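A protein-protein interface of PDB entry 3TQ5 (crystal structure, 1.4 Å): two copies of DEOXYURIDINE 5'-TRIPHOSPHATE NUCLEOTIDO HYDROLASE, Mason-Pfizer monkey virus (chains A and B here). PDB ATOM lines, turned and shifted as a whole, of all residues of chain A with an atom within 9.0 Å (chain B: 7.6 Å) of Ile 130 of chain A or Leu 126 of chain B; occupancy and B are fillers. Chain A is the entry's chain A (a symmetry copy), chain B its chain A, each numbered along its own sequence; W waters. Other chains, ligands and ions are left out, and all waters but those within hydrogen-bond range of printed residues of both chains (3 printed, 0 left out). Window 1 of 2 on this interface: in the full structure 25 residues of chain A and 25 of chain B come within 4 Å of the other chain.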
ATOM      1  N   ASN A  71      -8.479  -9.624  19.725  1.00  0.00           N
ATOM      2  CA  ASN A  71      -8.465  -8.257  20.230  1.00  0.00           C
ATOM      3  C   ASN A  71      -8.753  -8.123  21.716  1.00  0.00           C
ATOM      4  O   ASN A  71      -9.125  -7.035  22.152  1.00  0.00           O
ATOM      5  CB  ASN A  71      -9.446  -7.368  19.461  1.00  0.00           C
ATOM      6  CG  ASN A  71      -9.222  -7.460  17.952  1.00  0.00           C
ATOM      7  OD1 ASN A  71      -8.091  -7.275  17.485  1.00  0.00           O
ATOM      8  ND2 ASN A  71     -10.284  -7.755  17.196  1.00  0.00           N
ATOM      9  N   THR A  72      -8.593  -9.228  22.459  1.00  0.00           N
ATOM     10  CA  THR A  72      -8.781  -9.158  23.937  1.00  0.00           C
ATOM     11  C   THR A  72      -7.586  -9.719  24.666  1.00  0.00           C
ATOM     12  O   THR A  72      -6.806 -10.550  24.086  1.00  0.00           O
ATOM     13  CB  THR A  72     -10.013  -9.972  24.458  1.00  0.00           C
ATOM     14  OG1 THR A  72      -9.743 -11.369  24.343  1.00  0.00           O
ATOM     15  CG2 THR A  72     -11.298  -9.608  23.646  1.00  0.00           C
ATOM     16  N   PHE A  73      -7.415  -9.323  25.931  1.00  0.00           N
ATOM     17  CA  PHE A  73      -6.487 -10.088  26.792  1.00  0.00           C
ATOM     18  C   PHE A  73      -7.258 -10.338  28.097  1.00  0.00           C
ATOM     19  O   PHE A  73      -8.378  -9.859  28.280  1.00  0.00           O
ATOM     20  CB  PHE A  73      -5.196  -9.295  27.052  1.00  0.00           C
ATOM     21  CG  PHE A  73      -5.364  -8.116  28.000  1.00  0.00           C
ATOM     22  CD1 PHE A  73      -5.039  -8.242  29.380  1.00  0.00           C
ATOM     23  CD2 PHE A  73      -5.812  -6.900  27.538  1.00  0.00           C
ATOM     24  CE1 PHE A  73      -5.172  -7.147  30.245  1.00  0.00           C
ATOM     25  CE2 PHE A  73      -5.961  -5.787  28.429  1.00  0.00           C
ATOM     26  CZ  PHE A  73      -5.648  -5.916  29.767  1.00  0.00           C
ATOM     27  N   LEU A 127     -10.526  -8.008  28.565  1.00  0.00           N
ATOM     28  CA  LEU A 127     -10.388  -6.580  28.331  1.00  0.00           C
ATOM     29  C   LEU A 127      -9.852  -6.355  26.932  1.00  0.00           C
ATOM     30  O   LEU A 127      -9.217  -7.252  26.330  1.00  0.00           O
ATOM     31  CB  LEU A 127      -9.424  -5.950  29.322  1.00  0.00           C
ATOM     32  CG  LEU A 127     -10.027  -5.813  30.734  1.00  0.00           C
ATOM     33  CD1 LEU A 127      -8.910  -5.583  31.712  1.00  0.00           C
ATOM     34  CD2 LEU A 127     -11.079  -4.709  30.836  1.00  0.00           C
ATOM     35  N   PRO A 128     -10.155  -5.176  26.378  1.00  0.00           N
ATOM     36  CA  PRO A 128      -9.693  -4.870  25.039  1.00  0.00           C
ATOM     37  C   PRO A 128      -8.197  -4.738  25.023  1.00  0.00           C
ATOM     38  O   PRO A 128      -7.577  -4.229  25.953  1.00  0.00           O
ATOM     39  CB  PRO A 128     -10.341  -3.511  24.724  1.00  0.00           C
ATOM     40  CG  PRO A 128     -10.603  -2.918  26.031  1.00  0.00           C
ATOM     41  CD  PRO A 128     -10.923  -4.064  26.964  1.00  0.00           C
ATOM     42  N   LEU A 129      -7.635  -5.275  23.949  1.00  0.00           N
ATOM     43  CA  LEU A 129      -6.206  -5.198  23.728  1.00  0.00           C
ATOM     44  C   LEU A 129      -6.011  -4.047  22.744  1.00  0.00           C
ATOM     45  O   LEU A 129      -6.361  -4.143  21.555  1.00  0.00           O
ATOM     46  CB  LEU A 129      -5.757  -6.539  23.182  1.00  0.00           C
ATOM     47  CG  LEU A 129      -4.275  -6.636  22.883  1.00  0.00           C
ATOM     48  CD1 LEU A 129      -3.441  -6.289  24.057  1.00  0.00           C
ATOM     49  CD2 LEU A 129      -3.934  -8.084  22.434  1.00  0.00           C
ATOM     50  N   ILE A 130      -5.484  -2.943  23.260  1.00  0.00           N
ATOM     51  CA  ILE A 130      -5.232  -1.739  22.488  1.00  0.00           C
ATOM     52  C   ILE A 130      -3.983  -1.901  21.651  1.00  0.00           C
ATOM     53  O   ILE A 130      -2.955  -2.342  22.143  1.00  0.00           O
ATOM     54  CB  ILE A 130      -5.044  -0.565  23.474  1.00  0.00           C
ATOM     55  CG1 ILE A 130      -6.420  -0.180  24.034  1.00  0.00           C
ATOM     56  CG2 ILE A 130      -4.393   0.681  22.806  1.00  0.00           C
ATOM     57  CD1 ILE A 130      -6.348   0.932  25.074  1.00  0.00           C
ATOM     58  N   GLU A 131      -4.062  -1.474  20.388  1.00  0.00           N
ATOM     59  CA  GLU A 131      -2.892  -1.429  19.534  1.00  0.00           C
ATOM     60  C   GLU A 131      -2.026  -0.187  19.776  1.00  0.00           C
ATOM     61  O   GLU A 131      -2.510   0.894  20.116  1.00  0.00           O
ATOM     62  CB  GLU A 131      -3.367  -1.520  18.081  1.00  0.00           C
ATOM     63  CG  GLU A 131      -4.128  -2.813  17.796  1.00  0.00           C
ATOM     64  N   THR A 132      -0.712  -0.383  19.710  1.00  0.00           N
ATOM     65  CA  THR A 132       0.251   0.726  19.812  1.00  0.00           C
ATOM     66  C   THR A 132       1.367   0.451  18.785  1.00  0.00           C
ATOM     67  O   THR A 132       1.446  -0.646  18.235  1.00  0.00           O
ATOM     68  CB  THR A 132       0.879   0.856  21.239  1.00  0.00           C
ATOM     69  OG1 THR A 132       1.883  -0.160  21.439  1.00  0.00           O
ATOM     70  CG2 THR A 132      -0.177   0.728  22.357  1.00  0.00           C
ATOM     71  N   ASP A 133       2.222   1.431  18.546  1.00  0.00           N
ATOM     72  CA  ASP A 133       3.339   1.290  17.626  1.00  0.00           C
ATOM     73  C   ASP A 133       4.589   0.791  18.345  1.00  0.00           C
ATOM     74  O   ASP A 133       5.674   0.751  17.747  1.00  0.00           O
ATOM     75  CB  ASP A 133       3.664   2.646  16.993  1.00  0.00           C
ATOM     76  CG  ASP A 133       2.725   3.015  15.851  1.00  0.00           C
ATOM     77  OD1 ASP A 133       2.700   4.209  15.482  1.00  0.00           O
ATOM     78  OD2 ASP A 133       2.030   2.127  15.313  1.00  0.00           O
ATOM     79  N   ASN A 134       4.476   0.428  19.637  1.00  0.00           N
ATOM     80  CA  ASN A 134       5.679  -0.038  20.307  1.00  0.00           C
ATOM     81  C   ASN A 134       6.272  -1.210  19.528  1.00  0.00           C
ATOM     82  O   ASN A 134       5.539  -2.066  19.032  1.00  0.00           O
ATOM     83  CB  ASN A 134       5.444  -0.436  21.770  1.00  0.00           C
ATOM     84  CG  ASN A 134       4.958   0.730  22.635  1.00  0.00           C
ATOM     85  OD1 ASN A 134       3.748   1.034  22.660  1.00  0.00           O
ATOM     86  ND2 ASN A 134       5.858   1.304  23.423  1.00  0.00           N
ATOM     87  N   ILE B  28       7.093   6.358  26.924  1.00  0.00           N
ATOM     88  CA  ILE B  28       6.524   5.045  26.866  1.00  0.00           C
ATOM     89  C   ILE B  28       6.671   4.411  25.468  1.00  0.00           C
ATOM     90  O   ILE B  28       6.671   3.189  25.315  1.00  0.00           O
ATOM     91  CB  ILE B  28       5.076   5.084  27.410  1.00  0.00           C
ATOM     92  CG1 ILE B  28       5.141   4.866  28.936  1.00  0.00           C
ATOM     93  CG2 ILE B  28       4.195   4.059  26.735  1.00  0.00           C
ATOM     94  CD1 ILE B  28       4.032   5.496  29.676  1.00  0.00           C
ATOM     95  N   LEU B  31       9.290   1.689  25.059  1.00  0.00           N
ATOM     96  CA  LEU B  31       9.086   0.335  25.607  1.00  0.00           C
ATOM     97  C   LEU B  31       8.844  -0.656  24.506  1.00  0.00           C
ATOM     98  O   LEU B  31       8.323  -0.308  23.431  1.00  0.00           O
ATOM     99  CB  LEU B  31       7.873   0.297  26.555  1.00  0.00           C
ATOM    100  CG  LEU B  31       8.007   1.206  27.779  1.00  0.00           C
ATOM    101  CD1 LEU B  31       6.732   1.134  28.658  1.00  0.00           C
ATOM    102  CD2 LEU B  31       9.262   0.807  28.587  1.00  0.00           C
ATOM    103  N   ARG B  33       7.295  -4.692  23.364  1.00  0.00           N
ATOM    104  CA  ARG B  33       6.335  -5.754  23.605  1.00  0.00           C
ATOM    105  C   ARG B  33       7.117  -7.021  23.256  1.00  0.00           C
ATOM    106  O   ARG B  33       7.856  -7.032  22.247  1.00  0.00           O
ATOM    107  CB  ARG B  33       5.181  -5.541  22.621  1.00  0.00           C
ATOM    108  CG  ARG B  33       3.883  -6.074  23.048  1.00  0.00           C
ATOM    109  CD  ARG B  33       2.768  -5.724  22.077  1.00  0.00           C
ATOM    110  NE  ARG B  33       2.300  -4.320  22.170  1.00  0.00           N
ATOM    111  CZ  ARG B  33       1.530  -3.809  23.134  1.00  0.00           C
ATOM    112  NH1 ARG B  33       1.153  -4.553  24.178  1.00  0.00           N
ATOM    113  NH2 ARG B  33       1.164  -2.525  23.078  1.00  0.00           N
ATOM    114  N   PRO B  36       3.961  -9.951  19.413  1.00  0.00           N
ATOM    115  CA  PRO B  36       2.740  -9.238  19.009  1.00  0.00           C
ATOM    116  C   PRO B  36       1.439  -9.486  19.824  1.00  0.00           C
ATOM    117  O   PRO B  36       0.577  -8.622  19.829  1.00  0.00           O
ATOM    118  CB  PRO B  36       2.563  -9.623  17.522  1.00  0.00           C
ATOM    119  CG  PRO B  36       3.513 -10.765  17.265  1.00  0.00           C
ATOM    120  CD  PRO B  36       4.610 -10.643  18.273  1.00  0.00           C
ATOM    121  N   SER B  38       1.275 -10.082  23.092  1.00  0.00           N
ATOM    122  CA  SER B  38       1.549  -9.723  24.508  1.00  0.00           C
ATOM    123  C   SER B  38       0.722  -8.535  24.899  1.00  0.00           C
ATOM    124  O   SER B  38       0.702  -7.526  24.205  1.00  0.00           O
ATOM    125  CB  SER B  38       3.017  -9.359  24.748  1.00  0.00           C
ATOM    126  OG  SER B  38       3.835 -10.489  24.464  1.00  0.00           O
ATOM    127  N   ALA B  39       0.049  -8.646  26.036  1.00  0.00           N
ATOM    128  CA  ALA B  39      -0.812  -7.582  26.467  1.00  0.00           C
ATOM    129  C   ALA B  39       0.030  -6.438  26.989  1.00  0.00           C
ATOM    130  O   ALA B  39      -0.400  -5.293  26.903  1.00  0.00           O
ATOM    131  CB  ALA B  39      -1.714  -8.096  27.536  1.00  0.00           C
ATOM    132  N   GLY B  40       1.183  -6.732  27.585  1.00  0.00           N
ATOM    133  CA  GLY B  40       1.918  -5.686  28.324  1.00  0.00           C
ATOM    134  C   GLY B  40       3.194  -5.278  27.654  1.00  0.00           C
ATOM    135  O   GLY B  40       3.754  -6.033  26.844  1.00  0.00           O
ATOM    136  N   LEU B  41       3.600  -4.051  27.994  1.00  0.00           N
ATOM    137  CA  LEU B  41       4.898  -3.512  27.589  1.00  0.00           C
ATOM    138  C   LEU B  41       5.890  -3.782  28.721  1.00  0.00           C
ATOM    139  O   LEU B  41       5.623  -3.478  29.876  1.00  0.00           O
ATOM    140  CB  LEU B  41       4.805  -2.010  27.314  1.00  0.00           C
ATOM    141  CG  LEU B  41       3.841  -1.617  26.198  1.00  0.00           C
ATOM    142  CD1 LEU B  41       3.502  -0.045  26.223  1.00  0.00           C
ATOM    143  CD2 LEU B  41       4.417  -2.003  24.866  1.00  0.00           C
ATOM    144  N   PRO B  67       3.750  11.114  29.588  1.00  0.00           N
ATOM    145  CA  PRO B  67       2.333  10.720  29.669  1.00  0.00           C
ATOM    146  C   PRO B  67       1.916   9.643  28.692  1.00  0.00           C
ATOM    147  O   PRO B  67       2.775   9.101  27.975  1.00  0.00           O
ATOM    148  CB  PRO B  67       1.606  12.050  29.365  1.00  0.00           C
ATOM    149  CG  PRO B  67       2.556  12.675  28.271  1.00  0.00           C
ATOM    150  CD  PRO B  67       3.950  12.385  28.858  1.00  0.00           C
ATOM    151  N   LEU B  68       0.632   9.298  28.707  1.00  0.00           N
ATOM    152  CA  LEU B  68       0.148   8.179  27.953  1.00  0.00           C
ATOM    153  C   LEU B  68      -0.554   8.671  26.706  1.00  0.00           C
ATOM    154  O   LEU B  68      -0.833   9.869  26.576  1.00  0.00           O
ATOM    155  CB  LEU B  68      -0.811   7.361  28.812  1.00  0.00           C
ATOM    156  CG  LEU B  68      -0.217   6.845  30.133  1.00  0.00           C
ATOM    157  CD1 LEU B  68      -1.075   5.758  30.628  1.00  0.00           C
ATOM    158  CD2 LEU B  68       1.138   6.328  30.005  1.00  0.00           C
ATOM    159  N   PRO B  69      -0.828   7.756  25.765  1.00  0.00           N
ATOM    160  CA  PRO B  69      -1.535   8.141  24.538  1.00  0.00           C
ATOM    161  C   PRO B  69      -2.922   8.671  24.863  1.00  0.00           C
ATOM    162  O   PRO B  69      -3.523   8.261  25.885  1.00  0.00           O
ATOM    163  CB  PRO B  69      -1.643   6.809  23.782  1.00  0.00           C
ATOM    164  CG  PRO B  69      -0.507   5.979  24.266  1.00  0.00           C
ATOM    165  CD  PRO B  69      -0.445   6.326  25.756  1.00  0.00           C
ATOM    166  N   PRO B  70      -3.473   9.596  24.052  1.00  0.00           N
ATOM    167  CA  PRO B  70      -4.794  10.139  24.387  1.00  0.00           C
ATOM    168  C   PRO B  70      -5.850   9.041  24.647  1.00  0.00           C
ATOM    169  O   PRO B  70      -5.838   7.968  24.022  1.00  0.00           O
ATOM    170  CB  PRO B  70      -5.164  11.018  23.168  1.00  0.00           C
ATOM    171  CG  PRO B  70      -4.119  10.789  22.215  1.00  0.00           C
ATOM    172  CD  PRO B  70      -2.918  10.201  22.820  1.00  0.00           C
ATOM    173  N   ASN B  71      -6.740   9.320  25.591  1.00  0.00           N
ATOM    174  CA  ASN B  71      -7.861   8.441  25.901  1.00  0.00           C
ATOM    175  C   ASN B  71      -7.471   7.096  26.490  1.00  0.00           C
ATOM    176  O   ASN B  71      -8.278   6.169  26.437  1.00  0.00           O
ATOM    177  CB  ASN B  71      -8.736   8.199  24.669  1.00  0.00           C
ATOM    178  CG  ASN B  71      -9.160   9.513  24.014  1.00  0.00           C
ATOM    179  OD1 ASN B  71      -9.694  10.396  24.695  1.00  0.00           O
ATOM    180  ND2 ASN B  71      -8.914   9.649  22.707  1.00  0.00           N
ATOM    181  N   THR B  72      -6.242   7.008  27.022  1.00  0.00           N
ATOM    182  CA  THR B  72      -5.816   5.744  27.689  1.00  0.00           C
ATOM    183  C   THR B  72      -5.298   6.010  29.081  1.00  0.00           C
ATOM    184  O   THR B  72      -4.853   7.167  29.395  1.00  0.00           O
ATOM    185  CB  THR B  72      -4.660   4.994  26.946  1.00  0.00           C
ATOM    186  OG1 THR B  72      -3.445   5.733  27.088  1.00  0.00           O
ATOM    187  CG2 THR B  72      -5.001   4.817  25.431  1.00  0.00           C
ATOM    188  N   PHE B  73      -5.310   4.979  29.932  1.00  0.00           N
ATOM    189  CA  PHE B  73      -4.510   5.078  31.172  1.00  0.00           C
ATOM    190  C   PHE B  73      -3.726   3.760  31.255  1.00  0.00           C
ATOM    191  O   PHE B  73      -3.899   2.860  30.432  1.00  0.00           O
ATOM    192  CB  PHE B  73      -5.418   5.263  32.399  1.00  0.00           C
ATOM    193  CG  PHE B  73      -6.190   4.015  32.802  1.00  0.00           C
ATOM    194  CD1 PHE B  73      -5.710   3.166  33.839  1.00  0.00           C
ATOM    195  CD2 PHE B  73      -7.379   3.695  32.188  1.00  0.00           C
ATOM    196  CE1 PHE B  73      -6.436   2.031  34.223  1.00  0.00           C
ATOM    197  CE2 PHE B  73      -8.112   2.526  32.574  1.00  0.00           C
ATOM    198  CZ  PHE B  73      -7.640   1.704  33.577  1.00  0.00           C
ATOM    199  N   GLY B  74      -2.832   3.680  32.223  1.00  0.00           N
ATOM    200  CA  GLY B  74      -1.951   2.524  32.321  1.00  0.00           C
ATOM    201  C   GLY B  74      -2.163   1.805  33.628  1.00  0.00           C
ATOM    202  O   GLY B  74      -2.605   2.373  34.662  1.00  0.00           O
ATOM    203  N   LEU B  75      -1.911   0.497  33.559  1.00  0.00           N
ATOM    204  CA  LEU B  75      -1.831  -0.315  34.786  1.00  0.00           C
ATOM    205  C   LEU B  75      -0.518  -1.036  34.795  1.00  0.00           C
ATOM    206  O   LEU B  75      -0.168  -1.684  33.832  1.00  0.00           O
ATOM    207  CB  LEU B  75      -2.862  -1.433  34.831  1.00  0.00           C
ATOM    208  CG  LEU B  75      -4.319  -1.151  35.120  1.00  0.00           C
ATOM    209  CD1 LEU B  75      -5.057  -2.473  35.031  1.00  0.00           C
ATOM    210  CD2 LEU B  75      -4.595  -0.469  36.479  1.00  0.00           C
ATOM    211  N   ILE B  76       0.226  -0.881  35.879  1.00  0.00           N
ATOM    212  CA  ILE B  76       1.432  -1.658  36.137  1.00  0.00           C
ATOM    213  C   ILE B  76       1.060  -2.953  36.799  1.00  0.00           C
ATOM    214  O   ILE B  76       0.397  -2.916  37.800  1.00  0.00           O
ATOM    215  CB  ILE B  76       2.338  -0.875  37.113  1.00  0.00           C
ATOM    216  CG1 ILE B  76       2.509   0.543  36.593  1.00  0.00           C
ATOM    217  CG2 ILE B  76       3.691  -1.563  37.232  1.00  0.00           C
ATOM    218  CD1 ILE B  76       3.078   0.536  35.246  1.00  0.00           C
ATOM    219  N   ILE B  94      -1.594   4.325  36.309  1.00  0.00           N
ATOM    220  CA  ILE B  94      -0.828   5.425  35.723  1.00  0.00           C
ATOM    221  C   ILE B  94      -1.839   6.392  35.060  1.00  0.00           C
ATOM    222  O   ILE B  94      -2.513   6.037  34.083  1.00  0.00           O
ATOM    223  CB  ILE B  94       0.168   4.928  34.648  1.00  0.00           C
ATOM    224  CG1 ILE B  94       1.056   3.765  35.138  1.00  0.00           C
ATOM    225  CG2 ILE B  94       1.015   6.097  34.147  1.00  0.00           C
ATOM    226  CD1 ILE B  94       1.845   4.057  36.515  1.00  0.00           C
ATOM    227  N   GLN B 123       5.087  -5.151  33.885  1.00  0.00           N
ATOM    228  CA  GLN B 123       4.599  -4.835  32.565  1.00  0.00           C
ATOM    229  C   GLN B 123       3.585  -3.707  32.662  1.00  0.00           C
ATOM    230  O   GLN B 123       2.846  -3.620  33.649  1.00  0.00           O
ATOM    231  CB  GLN B 123       4.003  -6.082  31.857  1.00  0.00           C
ATOM    232  CG  GLN B 123       2.830  -6.752  32.621  1.00  0.00           C
ATOM    233  CD  GLN B 123       2.480  -8.037  31.933  1.00  0.00           C
ATOM    234  OE1 GLN B 123       2.193  -8.036  30.740  1.00  0.00           O
ATOM    235  NE2 GLN B 123       2.514  -9.131  32.687  1.00  0.00           N
ATOM    236  N   LEU B 124       3.514  -2.880  31.612  1.00  0.00           N
ATOM    237  CA  LEU B 124       2.554  -1.818  31.558  1.00  0.00           C
ATOM    238  C   LEU B 124       1.445  -2.218  30.582  1.00  0.00           C
ATOM    239  O   LEU B 124       1.712  -2.498  29.401  1.00  0.00           O
ATOM    240  CB  LEU B 124       3.256  -0.567  31.027  1.00  0.00           C
ATOM    241  CG  LEU B 124       2.329   0.637  30.887  1.00  0.00           C
ATOM    242  CD1 LEU B 124       1.895   1.113  32.266  1.00  0.00           C
ATOM    243  CD2 LEU B 124       3.148   1.802  30.223  1.00  0.00           C
ATOM    244  N   ILE B 125       0.207  -2.231  31.077  1.00  0.00           N
ATOM    245  CA  ILE B 125      -0.982  -2.508  30.244  1.00  0.00           C
ATOM    246  C   ILE B 125      -1.652  -1.148  29.956  1.00  0.00           C
ATOM    247  O   ILE B 125      -1.762  -0.328  30.863  1.00  0.00           O
ATOM    248  CB  ILE B 125      -1.932  -3.447  31.011  1.00  0.00           C
ATOM    249  CG1 ILE B 125      -1.590  -4.964  30.760  1.00  0.00           C
ATOM    250  CG2 ILE B 125      -3.408  -3.130  30.694  1.00  0.00           C
ATOM    251  CD1 ILE B 125      -0.348  -5.434  31.299  1.00  0.00           C
ATOM    252  N   LEU B 126      -2.114  -0.924  28.738  1.00  0.00           N
ATOM    253  CA  LEU B 126      -2.796   0.326  28.368  1.00  0.00           C
ATOM    254  C   LEU B 126      -4.283   0.004  28.253  1.00  0.00           C
ATOM    255  O   LEU B 126      -4.669  -0.991  27.621  1.00  0.00           O
ATOM    256  CB  LEU B 126      -2.264   0.847  27.048  1.00  0.00           C
ATOM    257  CG  LEU B 126      -0.827   1.370  27.183  1.00  0.00           C
ATOM    258  CD1 LEU B 126      -0.410   1.921  25.808  1.00  0.00           C
ATOM    259  CD2 LEU B 126      -0.680   2.540  28.170  1.00  0.00           C
ATOM    260  N   LEU B 127      -5.122   0.845  28.830  1.00  0.00           N
ATOM    261  CA  LEU B 127      -6.550   0.578  28.832  1.00  0.00           C
ATOM    262  C   LEU B 127      -7.296   1.855  28.501  1.00  0.00           C
ATOM    263  O   LEU B 127      -6.768   2.977  28.683  1.00  0.00           O
ATOM    264  CB  LEU B 127      -7.017   0.088  30.193  1.00  0.00           C
ATOM    265  CG  LEU B 127      -6.593  -1.367  30.479  1.00  0.00           C
ATOM    266  CD1 LEU B 127      -6.720  -1.621  31.954  1.00  0.00           C
ATOM    267  CD2 LEU B 127      -7.386  -2.396  29.676  1.00  0.00           C
ATOM    268  N   PRO B 128      -8.506   1.695  27.956  1.00  0.00           N
ATOM    269  CA  PRO B 128      -9.293   2.859  27.599  1.00  0.00           C
ATOM    270  C   PRO B 128      -9.710   3.603  28.834  1.00  0.00           C
ATOM    271  O   PRO B 128     -10.016   3.025  29.873  1.00  0.00           O
ATOM    272  CB  PRO B 128     -10.532   2.268  26.902  1.00  0.00           C
ATOM    273  CG  PRO B 128     -10.630   0.908  27.420  1.00  0.00           C
ATOM    274  CD  PRO B 128      -9.213   0.438  27.658  1.00  0.00           C
ATOM    275  N   LEU B 129      -9.650   4.922  28.697  1.00  0.00           N
ATOM    276  CA  LEU B 129     -10.065   5.810  29.762  1.00  0.00           C
ATOM    277  C   LEU B 129     -11.479   6.252  29.390  1.00  0.00           C
ATOM    278  O   LEU B 129     -11.689   7.021  28.437  1.00  0.00           O
ATOM    279  CB  LEU B 129      -9.071   6.954  29.814  1.00  0.00           C
ATOM    280  CG  LEU B 129      -9.359   7.994  30.878  1.00  0.00           C
ATOM    281  CD1 LEU B 129      -9.480   7.397  32.228  1.00  0.00           C
ATOM    282  CD2 LEU B 129      -8.214   9.045  30.893  1.00  0.00           C
HETATM  283  O   HOH W   1      -4.995  -3.147  26.162  1.00  0.00           O
HETATM  284  O   HOH W   2       3.022  -2.826  19.917  1.00  0.00           O
HETATM  285  O   HOH W   3      -1.319  -2.122  24.513  1.00  0.00           O
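The backbone carbonyl oxygen (O) of Ile 28 of chain B lies within hydrogen-bond range of the side-chain amide nitrogen (ND2) of Asn 134 of chain A (2.8 Å).
O of Leu 31 of chain B lies within hydrogen-bond range of ND2 of Asn 134 of chain A (2.9 Å).
The side-chain hydroxyl (OG1) of Thr 132 of chain A sits at hydrogen-bond distance from the guanidinium group (NH2) of Arg 33 of chain B (3.0 Å).
O of Ser 38 of chain B is in hydrogen-bond range of NH1 of Arg 33 of chain B (3.0 Å).
The guanidinium group (NH1) of Arg 33 of chain B sits at hydrogen-bond distance from the backbone carbonyl oxygen (O) of Ala 39 of chain B (3.2 Å).
The backbone carbonyl oxygen of Leu 41 of chain B lies within hydrogen-bond range of the backbone NH of Leu 124 of chain B (2.8 Å).
The backbone NH (N) of Leu 129 of chain A is in hydrogen-bond range of the backbone carbonyl oxygen (O) of Asn 71 of chain A (2.9 Å).
The backbone carbonyl oxygen of Leu 127 of chain A is in hydrogen-bond range of the backbone NH of Phe 73 of chain A (2.8 Å).
The side-chain hydroxyl (OG1) of Thr 132 of chain A is in hydrogen-bond range of the side-chain amide oxygen (OD1) of Asn 134 of chain A.
Ala 39 of chain B touches Phe 73 of chain A.
CZ of Phe 73 of chain A touches CG2 of Ile 125 of chain B (3.7 Å).
Phe 73 of chain A touches Leu 127 of chain B (CE2 to CD2, 3.9 Å).
Pro 128 of chain A touches Pro 128 of chain B.
CA of Ala 39 of chain B touches CD1 of Leu 129 of chain A, at 3.8 Å.
Ile 130 of chain A touches Leu 126 of chain B.
Ile 130 of chain A touches Leu 127 of chain B (CD1 to C, 3.7 Å).
Ile 130 of chain A touches Pro 128 of chain B (CD1 to N, 3.7 Å).
Thr 132 of chain A touches Leu 126 of chain B (CG2 to CD1, 3.7 Å).
Asn 134 of chain A touches Leu 41 of chain B (CG to CD2, 3.6 Å).
Thr 72 of chain A touches none of the printed residues of chain B.
Printed residues of chain B within 4 Å of Leu 129 of chain A: Ala 39 (3.8 Å).
Ile 130 of chain A touches three residues of chain B.
Of the printed residues of chain B, Thr 132 of chain A touches Arg 33 (3.0 Å) and Leu 126 (3.7 Å).
Of the printed residues of chain A, Arg 33 of chain B touches Thr 132.
Of the printed residues of chain A, Leu 41 of chain B touches Asn 134 (3.6 Å).
Asn 71 of chain B touches none of the printed residues of chain A.
Of chain A, only Ile 130 and Thr 132 come within 4 Å of Leu 126 of chain B.
Leu 127 of chain B touches just these residues of chain A: Phe 73 and Ile 130.
Printed residues of chain A within 4 Å of Pro 128 of chain B: Pro 128 (3.98 Å) and Ile 130 (3.7 Å).
The nearest printed residue of chain A that does not touch Ala 39 of chain B is Ile 130 of chain A (6.2 Å).
Of the 11 printed residues of chain A, 6 touch a printed residue of chain B.
Along chain A the printed residues that touch a printed residue of chain B span positions 73 to 134.
Along chain B the printed residues that touch a printed residue of chain A span positions 28 to 128.
Among the printed residues, no Asp or Glu carboxylate lies within 4 Å of a Lys or Arg side-chain nitrogen of the other chain.
Phe 73 of chain A touches Leu 127 of chain B, but with the chains exchanged Leu 127 of chain A does not touch Phe 73 of chain B (7.6 Å).
Pro 128 of chain A touches its own counterpart, Pro 128 of chain B.
6 positions are printed for both chains.
Of the 13 pairs that touch across the chains among the printed residues, 1 has its exchanged pair printed and touching as well.
Water W1 lies within hydrogen-bond range of the backbone carbonyl oxygen of Leu 126 of chain B (2.6 Å), the backbone carbonyl oxygen of Pro 128 of chain A (2.8 Å) and the backbone NH of Ile 130 of chain A (2.9 Å).
Water W2 lies within hydrogen-bond range of the backbone carbonyl oxygen of Asn 134 of chain A (2.8 Å), the guanidinium group of Arg 33 of chain B (2.8 Å) and the backbone carbonyl oxygen of Thr 132 of chain A (3.2 Å).
Water W3 lies within hydrogen-bond range of O of Ile 130 of chain A (2.9 Å) and NH2 of Arg 33 of chain B (2.9 Å).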
